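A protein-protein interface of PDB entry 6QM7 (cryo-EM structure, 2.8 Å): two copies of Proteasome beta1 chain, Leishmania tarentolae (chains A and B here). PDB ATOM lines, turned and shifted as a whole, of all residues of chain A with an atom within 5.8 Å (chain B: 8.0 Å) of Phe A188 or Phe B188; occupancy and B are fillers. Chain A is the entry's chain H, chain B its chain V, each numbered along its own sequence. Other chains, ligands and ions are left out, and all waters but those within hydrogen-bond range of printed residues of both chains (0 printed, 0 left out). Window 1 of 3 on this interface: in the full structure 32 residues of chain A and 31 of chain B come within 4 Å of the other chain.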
ATOM      1  N   SER A 184     -41.561  -4.007 -18.428  1.00  0.00           N
ATOM      2  CA  SER A 184     -41.191  -5.435 -18.273  1.00  0.00           C
ATOM      3  C   SER A 184     -39.835  -5.735 -18.935  1.00  0.00           C
ATOM      4  O   SER A 184     -39.052  -6.518 -18.355  1.00  0.00           O
ATOM      5  CB  SER A 184     -42.301  -6.299 -18.850  1.00  0.00           C
ATOM      6  OG  SER A 184     -42.092  -7.678 -18.559  1.00  0.00           O
ATOM      7  N   GLY A 185     -39.594  -5.182 -20.122  1.00  0.00           N
ATOM      8  CA  GLY A 185     -38.393  -5.449 -20.929  1.00  0.00           C
ATOM      9  C   GLY A 185     -37.183  -4.670 -20.447  1.00  0.00           C
ATOM     10  O   GLY A 185     -36.077  -5.003 -20.884  1.00  0.00           O
ATOM     11  N   SER A 186     -37.362  -3.652 -19.609  1.00  0.00           N
ATOM     12  CA  SER A 186     -36.254  -2.805 -19.098  1.00  0.00           C
ATOM     13  C   SER A 186     -35.198  -3.693 -18.454  1.00  0.00           C
ATOM     14  O   SER A 186     -34.014  -3.441 -18.679  1.00  0.00           O
ATOM     15  CB  SER A 186     -36.717  -1.765 -18.106  1.00  0.00           C
ATOM     16  OG  SER A 186     -37.056  -2.353 -16.854  1.00  0.00           O
ATOM     17  N   ILE A 187     -35.632  -4.693 -17.694  1.00  0.00           N
ATOM     18  CA  ILE A 187     -34.748  -5.548 -16.852  1.00  0.00           C
ATOM     19  C   ILE A 187     -33.691  -6.236 -17.726  1.00  0.00           C
ATOM     20  O   ILE A 187     -32.596  -6.490 -17.208  1.00  0.00           O
ATOM     21  CB  ILE A 187     -35.583  -6.548 -16.023  1.00  0.00           C
ATOM     22  CG1 ILE A 187     -34.859  -6.949 -14.740  1.00  0.00           C
ATOM     23  CG2 ILE A 187     -36.001  -7.756 -16.841  1.00  0.00           C
ATOM     24  CD1 ILE A 187     -34.840  -5.843 -13.693  1.00  0.00           C
ATOM     25  N   PHE A 188     -33.991  -6.516 -18.989  1.00  0.00           N
ATOM     26  CA  PHE A 188     -33.048  -7.163 -19.938  1.00  0.00           C
ATOM     27  C   PHE A 188     -31.963  -6.180 -20.371  1.00  0.00           C
ATOM     28  O   PHE A 188     -30.818  -6.611 -20.597  1.00  0.00           O
ATOM     29  CB  PHE A 188     -33.813  -7.742 -21.126  1.00  0.00           C
ATOM     30  CG  PHE A 188     -34.773  -8.805 -20.674  1.00  0.00           C
ATOM     31  CD1 PHE A 188     -34.298 -10.029 -20.246  1.00  0.00           C
ATOM     32  CD2 PHE A 188     -36.125  -8.550 -20.565  1.00  0.00           C
ATOM     33  CE1 PHE A 188     -35.166 -11.000 -19.777  1.00  0.00           C
ATOM     34  CE2 PHE A 188     -36.997  -9.526 -20.101  1.00  0.00           C
ATOM     35  CZ  PHE A 188     -36.516 -10.752 -19.707  1.00  0.00           C
ATOM     36  N   LEU A 189     -32.288  -4.896 -20.410  1.00  0.00           N
ATOM     37  CA  LEU A 189     -31.415  -3.876 -21.025  1.00  0.00           C
ATOM     38  C   LEU A 189     -30.371  -3.319 -20.056  1.00  0.00           C
ATOM     39  O   LEU A 189     -29.338  -2.856 -20.567  1.00  0.00           O
ATOM     40  CB  LEU A 189     -32.302  -2.773 -21.600  1.00  0.00           C
ATOM     41  CG  LEU A 189     -33.205  -3.233 -22.735  1.00  0.00           C
ATOM     42  CD1 LEU A 189     -33.862  -2.035 -23.400  1.00  0.00           C
ATOM     43  CD2 LEU A 189     -32.419  -4.052 -23.746  1.00  0.00           C
ATOM     44  N   TYR A 190     -30.592  -3.330 -18.744  1.00  0.00           N
ATOM     45  CA  TYR A 190     -29.659  -2.671 -17.792  1.00  0.00           C
ATOM     46  C   TYR A 190     -28.235  -3.175 -18.025  1.00  0.00           C
ATOM     47  O   TYR A 190     -27.295  -2.364 -18.024  1.00  0.00           O
ATOM     48  CB  TYR A 190     -30.076  -2.890 -16.341  1.00  0.00           C
ATOM     49  CG  TYR A 190     -31.255  -2.044 -15.956  1.00  0.00           C
ATOM     50  CD1 TYR A 190     -31.158  -0.665 -15.873  1.00  0.00           C
ATOM     51  CD2 TYR A 190     -32.482  -2.631 -15.726  1.00  0.00           C
ATOM     52  CE1 TYR A 190     -32.260   0.106 -15.542  1.00  0.00           C
ATOM     53  CE2 TYR A 190     -33.593  -1.872 -15.398  1.00  0.00           C
ATOM     54  CZ  TYR A 190     -33.483  -0.501 -15.301  1.00  0.00           C
ATOM     55  OH  TYR A 190     -34.612   0.205 -14.986  1.00  0.00           O
ATOM     56  N   SER A 191     -28.094  -4.478 -18.243  1.00  0.00           N
ATOM     57  CA  SER A 191     -26.790  -5.147 -18.460  1.00  0.00           C
ATOM     58  C   SER A 191     -26.303  -4.865 -19.882  1.00  0.00           C
ATOM     59  O   SER A 191     -25.094  -4.758 -20.075  1.00  0.00           O
ATOM     60  CB  SER A 191     -26.893  -6.619 -18.181  1.00  0.00           C
ATOM     61  OG  SER A 191     -25.846  -7.027 -17.326  1.00  0.00           O
ATOM     62  N   PHE A 192     -27.225  -4.762 -20.836  1.00  0.00           N
ATOM     63  CA  PHE A 192     -26.946  -4.412 -22.251  1.00  0.00           C
ATOM     64  C   PHE A 192     -26.351  -3.005 -22.331  1.00  0.00           C
ATOM     65  O   PHE A 192     -25.376  -2.817 -23.080  1.00  0.00           O
ATOM     66  CB  PHE A 192     -28.220  -4.510 -23.088  1.00  0.00           C
ATOM     67  CG  PHE A 192     -28.015  -4.171 -24.534  1.00  0.00           C
ATOM     68  CD1 PHE A 192     -27.451  -5.095 -25.390  1.00  0.00           C
ATOM     69  CD2 PHE A 192     -28.355  -2.921 -25.027  1.00  0.00           C
ATOM     70  CE1 PHE A 192     -27.251  -4.783 -26.726  1.00  0.00           C
ATOM     71  CE2 PHE A 192     -28.142  -2.606 -26.361  1.00  0.00           C
ATOM     72  CZ  PHE A 192     -27.586  -3.539 -27.207  1.00  0.00           C
ATOM     73  N   HIS A 216     -33.298  -6.330 -28.390  1.00  0.00           N
ATOM     74  CA  HIS A 216     -32.667  -7.278 -27.435  1.00  0.00           C
ATOM     75  C   HIS A 216     -33.635  -7.565 -26.295  1.00  0.00           C
ATOM     76  O   HIS A 216     -33.678  -8.728 -25.841  1.00  0.00           O
ATOM     77  CB  HIS A 216     -31.292  -6.795 -26.973  1.00  0.00           C
ATOM     78  CG  HIS A 216     -30.234  -7.367 -27.841  1.00  0.00           C
ATOM     79  ND1 HIS A 216     -29.591  -6.631 -28.812  1.00  0.00           N
ATOM     80  CD2 HIS A 216     -29.782  -8.634 -27.943  1.00  0.00           C
ATOM     81  CE1 HIS A 216     -28.763  -7.422 -29.475  1.00  0.00           C
ATOM     82  NE2 HIS A 216     -28.859  -8.664 -28.959  1.00  0.00           N
ATOM     83  N   ALA A 217     -34.391  -6.563 -25.876  1.00  0.00           N
ATOM     84  CA  ALA A 217     -35.389  -6.697 -24.803  1.00  0.00           C
ATOM     85  C   ALA A 217     -36.528  -7.575 -25.298  1.00  0.00           C
ATOM     86  O   ALA A 217     -36.950  -8.477 -24.541  1.00  0.00           O
ATOM     87  CB  ALA A 217     -35.911  -5.350 -24.382  1.00  0.00           C
ATOM     88  N   ARG A 220     -36.320 -11.432 -25.608  1.00  0.00           N
ATOM     89  CA  ARG A 220     -36.339 -12.194 -24.340  1.00  0.00           C
ATOM     90  C   ARG A 220     -37.635 -11.945 -23.561  1.00  0.00           C
ATOM     91  O   ARG A 220     -38.136 -12.895 -22.956  1.00  0.00           O
ATOM     92  CB  ARG A 220     -35.125 -11.793 -23.499  1.00  0.00           C
ATOM     93  CG  ARG A 220     -33.802 -12.242 -24.096  1.00  0.00           C
ATOM     94  CD  ARG A 220     -33.687 -13.738 -23.973  1.00  0.00           C
ATOM     95  NE  ARG A 220     -32.443 -14.265 -24.484  1.00  0.00           N
ATOM     96  CZ  ARG A 220     -32.133 -15.550 -24.480  1.00  0.00           C
ATOM     97  NH1 ARG A 220     -32.977 -16.440 -23.987  1.00  0.00           N
ATOM     98  NH2 ARG A 220     -30.977 -15.948 -24.980  1.00  0.00           N
ATOM     99  N   ASP A 221     -38.139 -10.713 -23.528  1.00  0.00           N
ATOM    100  CA  ASP A 221     -39.431 -10.413 -22.861  1.00  0.00           C
ATOM    101  C   ASP A 221     -40.564 -10.951 -23.740  1.00  0.00           C
ATOM    102  O   ASP A 221     -40.674 -10.528 -24.908  1.00  0.00           O
ATOM    103  CB  ASP A 221     -39.578  -8.917 -22.574  1.00  0.00           C
ATOM    104  CG  ASP A 221     -40.675  -8.572 -21.574  1.00  0.00           C
ATOM    105  OD1 ASP A 221     -40.932  -9.406 -20.670  1.00  0.00           O
ATOM    106  OD2 ASP A 221     -41.263  -7.458 -21.700  1.00  0.00           O
ATOM    107  N   THR B  55     -28.413 -14.237  -6.460  1.00  0.00           N
ATOM    108  CA  THR B  55     -27.467 -15.305  -6.917  1.00  0.00           C
ATOM    109  C   THR B  55     -27.337 -15.239  -8.437  1.00  0.00           C
ATOM    110  O   THR B  55     -28.363 -15.092  -9.109  1.00  0.00           O
ATOM    111  CB  THR B  55     -27.942 -16.705  -6.496  1.00  0.00           C
ATOM    112  OG1 THR B  55     -27.949 -16.794  -5.070  1.00  0.00           O
ATOM    113  CG2 THR B  55     -27.089 -17.829  -7.049  1.00  0.00           C
ATOM    114  N   THR B  56     -26.115 -15.330  -8.940  1.00  0.00           N
ATOM    115  CA  THR B  56     -25.800 -15.354 -10.384  1.00  0.00           C
ATOM    116  C   THR B  56     -24.926 -16.567 -10.627  1.00  0.00           C
ATOM    117  O   THR B  56     -23.833 -16.599 -10.079  1.00  0.00           O
ATOM    118  CB  THR B  56     -25.049 -14.106 -10.856  1.00  0.00           C
ATOM    119  OG1 THR B  56     -25.755 -12.941 -10.436  1.00  0.00           O
ATOM    120  CG2 THR B  56     -24.898 -14.101 -12.361  1.00  0.00           C
ATOM    121  N   LEU B 181     -27.661 -19.986 -17.841  1.00  0.00           N
ATOM    122  CA  LEU B 181     -27.716 -18.906 -16.835  1.00  0.00           C
ATOM    123  C   LEU B 181     -28.618 -19.373 -15.698  1.00  0.00           C
ATOM    124  O   LEU B 181     -29.487 -20.233 -15.941  1.00  0.00           O
ATOM    125  CB  LEU B 181     -28.288 -17.666 -17.512  1.00  0.00           C
ATOM    126  CG  LEU B 181     -27.311 -16.764 -18.259  1.00  0.00           C
ATOM    127  CD1 LEU B 181     -26.208 -17.527 -18.930  1.00  0.00           C
ATOM    128  CD2 LEU B 181     -28.065 -15.968 -19.304  1.00  0.00           C
ATOM    129  N   GLY B 183     -30.168 -18.224 -11.354  1.00  0.00           N
ATOM    130  CA  GLY B 183     -30.236 -17.289 -10.221  1.00  0.00           C
ATOM    131  C   GLY B 183     -30.906 -15.971 -10.584  1.00  0.00           C
ATOM    132  O   GLY B 183     -31.005 -15.630 -11.766  1.00  0.00           O
ATOM    133  N   SER B 184     -31.361 -15.260  -9.561  1.00  0.00           N
ATOM    134  CA  SER B 184     -31.857 -13.865  -9.597  1.00  0.00           C
ATOM    135  C   SER B 184     -31.136 -13.050 -10.683  1.00  0.00           C
ATOM    136  O   SER B 184     -31.823 -12.345 -11.454  1.00  0.00           O
ATOM    137  CB  SER B 184     -31.687 -13.259  -8.217  1.00  0.00           C
ATOM    138  OG  SER B 184     -32.210 -11.936  -8.162  1.00  0.00           O
ATOM    139  N   GLY B 185     -29.806 -13.136 -10.733  1.00  0.00           N
ATOM    140  CA  GLY B 185     -28.949 -12.339 -11.628  1.00  0.00           C
ATOM    141  C   GLY B 185     -28.981 -12.822 -13.064  1.00  0.00           C
ATOM    142  O   GLY B 185     -28.467 -12.085 -13.918  1.00  0.00           O
ATOM    143  N   SER B 186     -29.517 -14.017 -13.331  1.00  0.00           N
ATOM    144  CA  SER B 186     -29.594 -14.605 -14.694  1.00  0.00           C
ATOM    145  C   SER B 186     -30.287 -13.623 -15.635  1.00  0.00           C
ATOM    146  O   SER B 186     -29.795 -13.435 -16.748  1.00  0.00           O
ATOM    147  CB  SER B 186     -30.308 -15.946 -14.721  1.00  0.00           C
ATOM    148  OG  SER B 186     -31.714 -15.811 -14.527  1.00  0.00           O
ATOM    149  N   ILE B 187     -31.384 -13.028 -15.174  1.00  0.00           N
ATOM    150  CA  ILE B 187     -32.313 -12.186 -15.980  1.00  0.00           C
ATOM    151  C   ILE B 187     -31.569 -10.990 -16.581  1.00  0.00           C
ATOM    152  O   ILE B 187     -32.075 -10.447 -17.577  1.00  0.00           O
ATOM    153  CB  ILE B 187     -33.512 -11.741 -15.122  1.00  0.00           C
ATOM    154  CG1 ILE B 187     -34.748 -11.483 -15.984  1.00  0.00           C
ATOM    155  CG2 ILE B 187     -33.166 -10.549 -14.242  1.00  0.00           C
ATOM    156  CD1 ILE B 187     -35.414 -12.762 -16.475  1.00  0.00           C
ATOM    157  N   PHE B 188     -30.438 -10.590 -16.000  1.00  0.00           N
ATOM    158  CA  PHE B 188     -29.596  -9.482 -16.507  1.00  0.00           C
ATOM    159  C   PHE B 188     -28.767  -9.959 -17.692  1.00  0.00           C
ATOM    160  O   PHE B 188     -28.576  -9.178 -18.641  1.00  0.00           O
ATOM    161  CB  PHE B 188     -28.764  -8.886 -15.377  1.00  0.00           C
ATOM    162  CG  PHE B 188     -29.652  -8.269 -14.329  1.00  0.00           C
ATOM    163  CD1 PHE B 188     -30.354  -7.110 -14.604  1.00  0.00           C
ATOM    164  CD2 PHE B 188     -29.876  -8.906 -13.118  1.00  0.00           C
ATOM    165  CE1 PHE B 188     -31.218  -6.575 -13.666  1.00  0.00           C
ATOM    166  CE2 PHE B 188     -30.732  -8.360 -12.172  1.00  0.00           C
ATOM    167  CZ  PHE B 188     -31.400  -7.191 -12.447  1.00  0.00           C
ATOM    168  N   LEU B 189     -28.374 -11.223 -17.685  1.00  0.00           N
ATOM    169  CA  LEU B 189     -27.356 -11.756 -18.618  1.00  0.00           C
ATOM    170  C   LEU B 189     -27.964 -12.230 -19.940  1.00  0.00           C
ATOM    171  O   LEU B 189     -27.203 -12.283 -20.905  1.00  0.00           O
ATOM    172  CB  LEU B 189     -26.617 -12.887 -17.912  1.00  0.00           C
ATOM    173  CG  LEU B 189     -25.822 -12.447 -16.693  1.00  0.00           C
ATOM    174  CD1 LEU B 189     -25.067 -13.614 -16.099  1.00  0.00           C
ATOM    175  CD2 LEU B 189     -24.867 -11.327 -17.063  1.00  0.00           C
ATOM    176  N   TYR B 190     -29.254 -12.549 -20.026  1.00  0.00           N
ATOM    177  CA  TYR B 190     -29.832 -13.116 -21.274  1.00  0.00           C
ATOM    178  C   TYR B 190     -29.537 -12.178 -22.437  1.00  0.00           C
ATOM    179  O   TYR B 190     -29.144 -12.655 -23.506  1.00  0.00           O
ATOM    180  CB  TYR B 190     -31.329 -13.388 -21.149  1.00  0.00           C
ATOM    181  CG  TYR B 190     -31.608 -14.605 -20.315  1.00  0.00           C
ATOM    182  CD1 TYR B 190     -31.236 -15.869 -20.751  1.00  0.00           C
ATOM    183  CD2 TYR B 190     -32.180 -14.482 -19.064  1.00  0.00           C
ATOM    184  CE1 TYR B 190     -31.441 -16.994 -19.964  1.00  0.00           C
ATOM    185  CE2 TYR B 190     -32.397 -15.596 -18.268  1.00  0.00           C
ATOM    186  CZ  TYR B 190     -32.025 -16.860 -18.712  1.00  0.00           C
ATOM    187  OH  TYR B 190     -32.256 -17.949 -17.909  1.00  0.00           O
ATOM    188  N   SER B 191     -29.674 -10.879 -22.205  1.00  0.00           N
ATOM    189  CA  SER B 191     -29.482  -9.825 -23.233  1.00  0.00           C
ATOM    190  C   SER B 191     -27.985  -9.579 -23.432  1.00  0.00           C
ATOM    191  O   SER B 191     -27.577  -9.228 -24.550  1.00  0.00           O
ATOM    192  CB  SER B 191     -30.209  -8.575 -22.841  1.00  0.00           C
ATOM    193  OG  SER B 191     -31.080  -8.179 -23.875  1.00  0.00           O
ATOM    194  N   PHE B 192     -27.202  -9.722 -22.369  1.00  0.00           N
ATOM    195  CA  PHE B 192     -25.724  -9.621 -22.405  1.00  0.00           C
ATOM    196  C   PHE B 192     -25.140 -10.708 -23.306  1.00  0.00           C
ATOM    197  O   PHE B 192     -24.227 -10.408 -24.086  1.00  0.00           O
ATOM    198  CB  PHE B 192     -25.140  -9.788 -21.009  1.00  0.00           C
ATOM    199  CG  PHE B 192     -23.652  -9.638 -20.984  1.00  0.00           C
ATOM    200  CD1 PHE B 192     -23.074  -8.383 -21.089  1.00  0.00           C
ATOM    201  CD2 PHE B 192     -22.841 -10.750 -20.865  1.00  0.00           C
ATOM    202  CE1 PHE B 192     -21.699  -8.244 -21.067  1.00  0.00           C
ATOM    203  CE2 PHE B 192     -21.464 -10.614 -20.858  1.00  0.00           C
ATOM    204  CZ  PHE B 192     -20.898  -9.361 -20.966  1.00  0.00           C
ATOM    205  N   PHE B 193     -25.631 -11.939 -23.159  1.00  0.00           N
ATOM    206  CA  PHE B 193     -25.192 -13.119 -23.941  1.00  0.00           C
ATOM    207  C   PHE B 193     -25.676 -12.954 -25.376  1.00  0.00           C
ATOM    208  O   PHE B 193     -24.848 -13.035 -26.282  1.00  0.00           O
ATOM    209  CB  PHE B 193     -25.683 -14.426 -23.316  1.00  0.00           C
ATOM    210  CG  PHE B 193     -24.724 -14.999 -22.309  1.00  0.00           C
ATOM    211  CD1 PHE B 193     -23.953 -16.105 -22.622  1.00  0.00           C
ATOM    212  CD2 PHE B 193     -24.567 -14.410 -21.070  1.00  0.00           C
ATOM    213  CE1 PHE B 193     -23.047 -16.620 -21.706  1.00  0.00           C
ATOM    214  CE2 PHE B 193     -23.670 -14.924 -20.148  1.00  0.00           C
ATOM    215  CZ  PHE B 193     -22.908 -16.032 -20.464  1.00  0.00           C
ATOM    216  N   ASP B 194     -26.966 -12.683 -25.570  1.00  0.00           N
ATOM    217  CA  ASP B 194     -27.565 -12.449 -26.910  1.00  0.00           C
ATOM    218  C   ASP B 194     -26.681 -11.506 -27.728  1.00  0.00           C
ATOM    219  O   ASP B 194     -26.513 -11.757 -28.934  1.00  0.00           O
ATOM    220  CB  ASP B 194     -28.979 -11.880 -26.795  1.00  0.00           C
ATOM    221  CG  ASP B 194     -30.059 -12.910 -26.469  1.00  0.00           C
ATOM    222  OD1 ASP B 194     -31.222 -12.485 -26.240  1.00  0.00           O
ATOM    223  OD2 ASP B 194     -29.742 -14.120 -26.432  1.00  0.00           O
ATOM    224  N   ALA B 213     -19.416 -11.481 -17.470  1.00  0.00           N
ATOM    225  CA  ALA B 213     -20.865 -11.741 -17.361  1.00  0.00           C
ATOM    226  C   ALA B 213     -21.252 -11.619 -15.901  1.00  0.00           C
ATOM    227  O   ALA B 213     -21.987 -10.695 -15.576  1.00  0.00           O
ATOM    228  CB  ALA B 213     -21.244 -13.096 -17.901  1.00  0.00           C
ATOM    229  N   VAL B 214     -20.721 -12.485 -15.049  1.00  0.00           N
ATOM    230  CA  VAL B 214     -21.087 -12.502 -13.609  1.00  0.00           C
ATOM    231  C   VAL B 214     -21.019 -11.076 -13.063  1.00  0.00           C
ATOM    232  O   VAL B 214     -21.948 -10.677 -12.355  1.00  0.00           O
ATOM    233  CB  VAL B 214     -20.202 -13.443 -12.788  1.00  0.00           C
ATOM    234  CG1 VAL B 214     -20.422 -13.236 -11.298  1.00  0.00           C
ATOM    235  CG2 VAL B 214     -20.468 -14.890 -13.147  1.00  0.00           C
ATOM    236  N   HIS B 216     -21.383  -8.215 -14.614  1.00  0.00           N
ATOM    237  CA  HIS B 216     -22.474  -7.393 -15.192  1.00  0.00           C
ATOM    238  C   HIS B 216     -23.772  -7.691 -14.458  1.00  0.00           C
ATOM    239  O   HIS B 216     -24.542  -6.750 -14.263  1.00  0.00           O
ATOM    240  CB  HIS B 216     -22.555  -7.560 -16.716  1.00  0.00           C
ATOM    241  CG  HIS B 216     -21.792  -6.478 -17.390  1.00  0.00           C
ATOM    242  ND1 HIS B 216     -20.570  -6.693 -17.974  1.00  0.00           N
ATOM    243  CD2 HIS B 216     -22.031  -5.152 -17.466  1.00  0.00           C
ATOM    244  CE1 HIS B 216     -20.098  -5.545 -18.428  1.00  0.00           C
ATOM    245  NE2 HIS B 216     -20.979  -4.588 -18.133  1.00  0.00           N
ATOM    246  N   ALA B 217     -23.978  -8.932 -14.054  1.00  0.00           N
ATOM    247  CA  ALA B 217     -25.195  -9.376 -13.347  1.00  0.00           C
ATOM    248  C   ALA B 217     -25.180  -8.865 -11.920  1.00  0.00           C
ATOM    249  O   ALA B 217     -26.253  -8.507 -11.438  1.00  0.00           O
ATOM    250  CB  ALA B 217     -25.279 -10.876 -13.320  1.00  0.00           C
ATOM    251  N   TYR B 218     -24.037  -8.918 -11.242  1.00  0.00           N
ATOM    252  CA  TYR B 218     -23.983  -8.622  -9.792  1.00  0.00           C
ATOM    253  C   TYR B 218     -23.901  -7.110  -9.600  1.00  0.00           C
ATOM    254  O   TYR B 218     -24.172  -6.647  -8.469  1.00  0.00           O
ATOM    255  CB  TYR B 218     -22.965  -9.497  -9.055  1.00  0.00           C
ATOM    256  CG  TYR B 218     -21.487  -9.189  -9.092  1.00  0.00           C
ATOM    257  CD1 TYR B 218     -20.938  -7.959  -9.419  1.00  0.00           C
ATOM    258  CD2 TYR B 218     -20.611 -10.167  -8.679  1.00  0.00           C
ATOM    259  CE1 TYR B 218     -19.569  -7.738  -9.409  1.00  0.00           C
ATOM    260  CE2 TYR B 218     -19.247  -9.961  -8.643  1.00  0.00           C
ATOM    261  CZ  TYR B 218     -18.717  -8.747  -9.017  1.00  0.00           C
ATOM    262  OH  TYR B 218     -17.363  -8.583  -8.968  1.00  0.00           O
ATOM    263  N   SER B 219     -23.592  -6.362 -10.655  1.00  0.00           N
ATOM    264  CA  SER B 219     -23.574  -4.878 -10.636  1.00  0.00           C
ATOM    265  C   SER B 219     -25.008  -4.353 -10.582  1.00  0.00           C
ATOM    266  O   SER B 219     -25.197  -3.277  -9.985  1.00  0.00           O
ATOM    267  CB  SER B 219     -22.820  -4.326 -11.806  1.00  0.00           C
ATOM    268  OG  SER B 219     -21.472  -4.791 -11.757  1.00  0.00           O
ATOM    269  N   ARG B 220     -25.969  -5.113 -11.114  1.00  0.00           N
ATOM    270  CA  ARG B 220     -27.397  -4.717 -11.190  1.00  0.00           C
ATOM    271  C   ARG B 220     -28.240  -5.484 -10.167  1.00  0.00           C
ATOM    272  O   ARG B 220     -29.067  -4.839  -9.519  1.00  0.00           O
ATOM    273  CB  ARG B 220     -27.885  -4.940 -12.621  1.00  0.00           C
ATOM    274  CG  ARG B 220     -27.263  -3.988 -13.630  1.00  0.00           C
ATOM    275  CD  ARG B 220     -27.846  -2.611 -13.411  1.00  0.00           C
ATOM    276  NE  ARG B 220     -27.321  -1.594 -14.298  1.00  0.00           N
ATOM    277  CZ  ARG B 220     -27.716  -0.337 -14.281  1.00  0.00           C
ATOM    278  NH1 ARG B 220     -28.633   0.063 -13.421  1.00  0.00           N
ATOM    279  NH2 ARG B 220     -27.188   0.532 -15.120  1.00  0.00           N
ATOM    280  N   ASP B 221     -28.068  -6.805 -10.050  1.00  0.00           N
ATOM    281  CA  ASP B 221     -28.779  -7.651  -9.055  1.00  0.00           C
ATOM    282  C   ASP B 221     -28.270  -7.305  -7.657  1.00  0.00           C
ATOM    283  O   ASP B 221     -27.042  -7.374  -7.440  1.00  0.00           O
ATOM    284  CB  ASP B 221     -28.581  -9.147  -9.309  1.00  0.00           C
ATOM    285  CG  ASP B 221     -29.567 -10.060  -8.567  1.00  0.00           C
ATOM    286  OD1 ASP B 221     -30.696  -9.593  -8.231  1.00  0.00           O
ATOM    287  OD2 ASP B 221     -29.224 -11.254  -8.348  1.00  0.00           O
ATOM    288  N   GLY B 222     -29.165  -6.886  -6.762  1.00  0.00           N
ATOM    289  CA  GLY B 222     -28.839  -6.642  -5.344  1.00  0.00           C
ATOM    290  C   GLY B 222     -28.556  -7.955  -4.635  1.00  0.00           C
ATOM    291  O   GLY B 222     -27.707  -7.981  -3.729  1.00  0.00           O
ATOM    292  N   SER B 223     -29.236  -9.016  -5.065  1.00  0.00           N
ATOM    293  CA  SER B 223     -29.185 -10.369  -4.459  1.00  0.00           C
ATOM    294  C   SER B 223     -27.898 -11.098  -4.865  1.00  0.00           C
ATOM    295  O   SER B 223     -27.642 -12.164  -4.287  1.00  0.00           O
ATOM    296  CB  SER B 223     -30.403 -11.174  -4.851  1.00  0.00           C
ATOM    297  OG  SER B 223     -31.522 -10.334  -5.112  1.00  0.00           O
ATOM    298  N   SER B 224     -27.149 -10.567  -5.840  1.00  0.00           N
ATOM    299  CA  SER B 224     -25.822 -11.068  -6.279  1.00  0.00           C
ATOM    300  C   SER B 224     -24.751 -10.074  -5.868  1.00  0.00           C
ATOM    301  O   SER B 224     -25.061  -8.874  -5.772  1.00  0.00           O
ATOM    302  CB  SER B 224     -25.758 -11.302  -7.760  1.00  0.00           C
ATOM    303  OG  SER B 224     -26.780 -12.190  -8.191  1.00  0.00           O
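Ile A187 touches Phe B188.
CD1 of Phe A188 touches O of Ile B187, at 3.5 Å.
Phe A188 touches Phe B188 (O to O, 3.9 Å).
Phe A188 touches Ser B191 (O to CB, 3.0 Å).
CD1 of Tyr A190 touches NH1 of Arg B220 (3.6 Å).
Phe B188 touches Ser A191 (O to CB, 3.1 Å).
CD2 of His A216 touches CB of Asp B194 (3.5 Å).
Tyr B190 touches Arg A220 (CB to NE, 3.6 Å).
Hydrophobic or aromatic side chains of chain B that line the printed part of chain A: Ile B187, Phe B188, Tyr B190 and His B216.
Along chain B the printed residues that touch a printed residue of chain A span positions 187 to 220.
Printed residues of chain A that touch a printed residue of chain B: Ile A187, Phe A188, Tyr A190, Ser A191, His A216 and Arg A220.
Along chain A the printed residues that touch a printed residue of chain B span positions 187 to 220.
Among the printed residues, 11 pairs touch across the chains.
Among the printed residues, Asp or Glu carboxylates within 4 Å of a Lys or Arg side-chain nitrogen of the other chain: Arg A220 with Asp B194 (2.6 Å).
Ile A187 touches Phe B188, and with the chains exchanged Phe A188 touches Ile B187.
Phe B188 touches its own counterpart, Phe A188.
Tyr A190 touches Arg B220, and with the chains exchanged Arg A220 touches Tyr B190.
Ser A191 touches His B216, and with the chains exchanged His A216 touches Ser B191.
13 positions are printed for both chains.
The side-chain hydroxyl of Ser A191 is in hydrogen-bond range of the backbone carbonyl oxygen of His B216 (3.3 Å).
The backbone carbonyl oxygen of His A216 lies within hydrogen-bond range of the side-chain hydroxyl of Ser B191.
NH2 of Arg A220 is in salt-bridge range of OD2 of Asp B194, at 2.6 Å.
Of chain B, only Ile B187, Phe B188 and Ser B191 come within 4 Å of Phe A188.
Gly B183 touches none of the printed residues of chain A.
Of the printed residues of chain A, Ile B187 touches Phe A188 (3.5 Å).
Printed residues of chain A within 4 Å of Tyr B190: Arg A220 (3.6 Å).
Printed residues of chain A within 4 Å of Asp B194: His A216 (3.5 Å) and Arg A220 (2.6 Å).
Of the printed residues of chain A, His B216 touches Ser A191.
Printed residues of chain A within 4 Å of Arg B220: Tyr A190.
The nearest residue of chain B that does not touch Phe A188 is Tyr B190 (4.6 Å).
The nearest residue of chain A that does not touch Phe B188 is Tyr A190 (4.6 Å).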
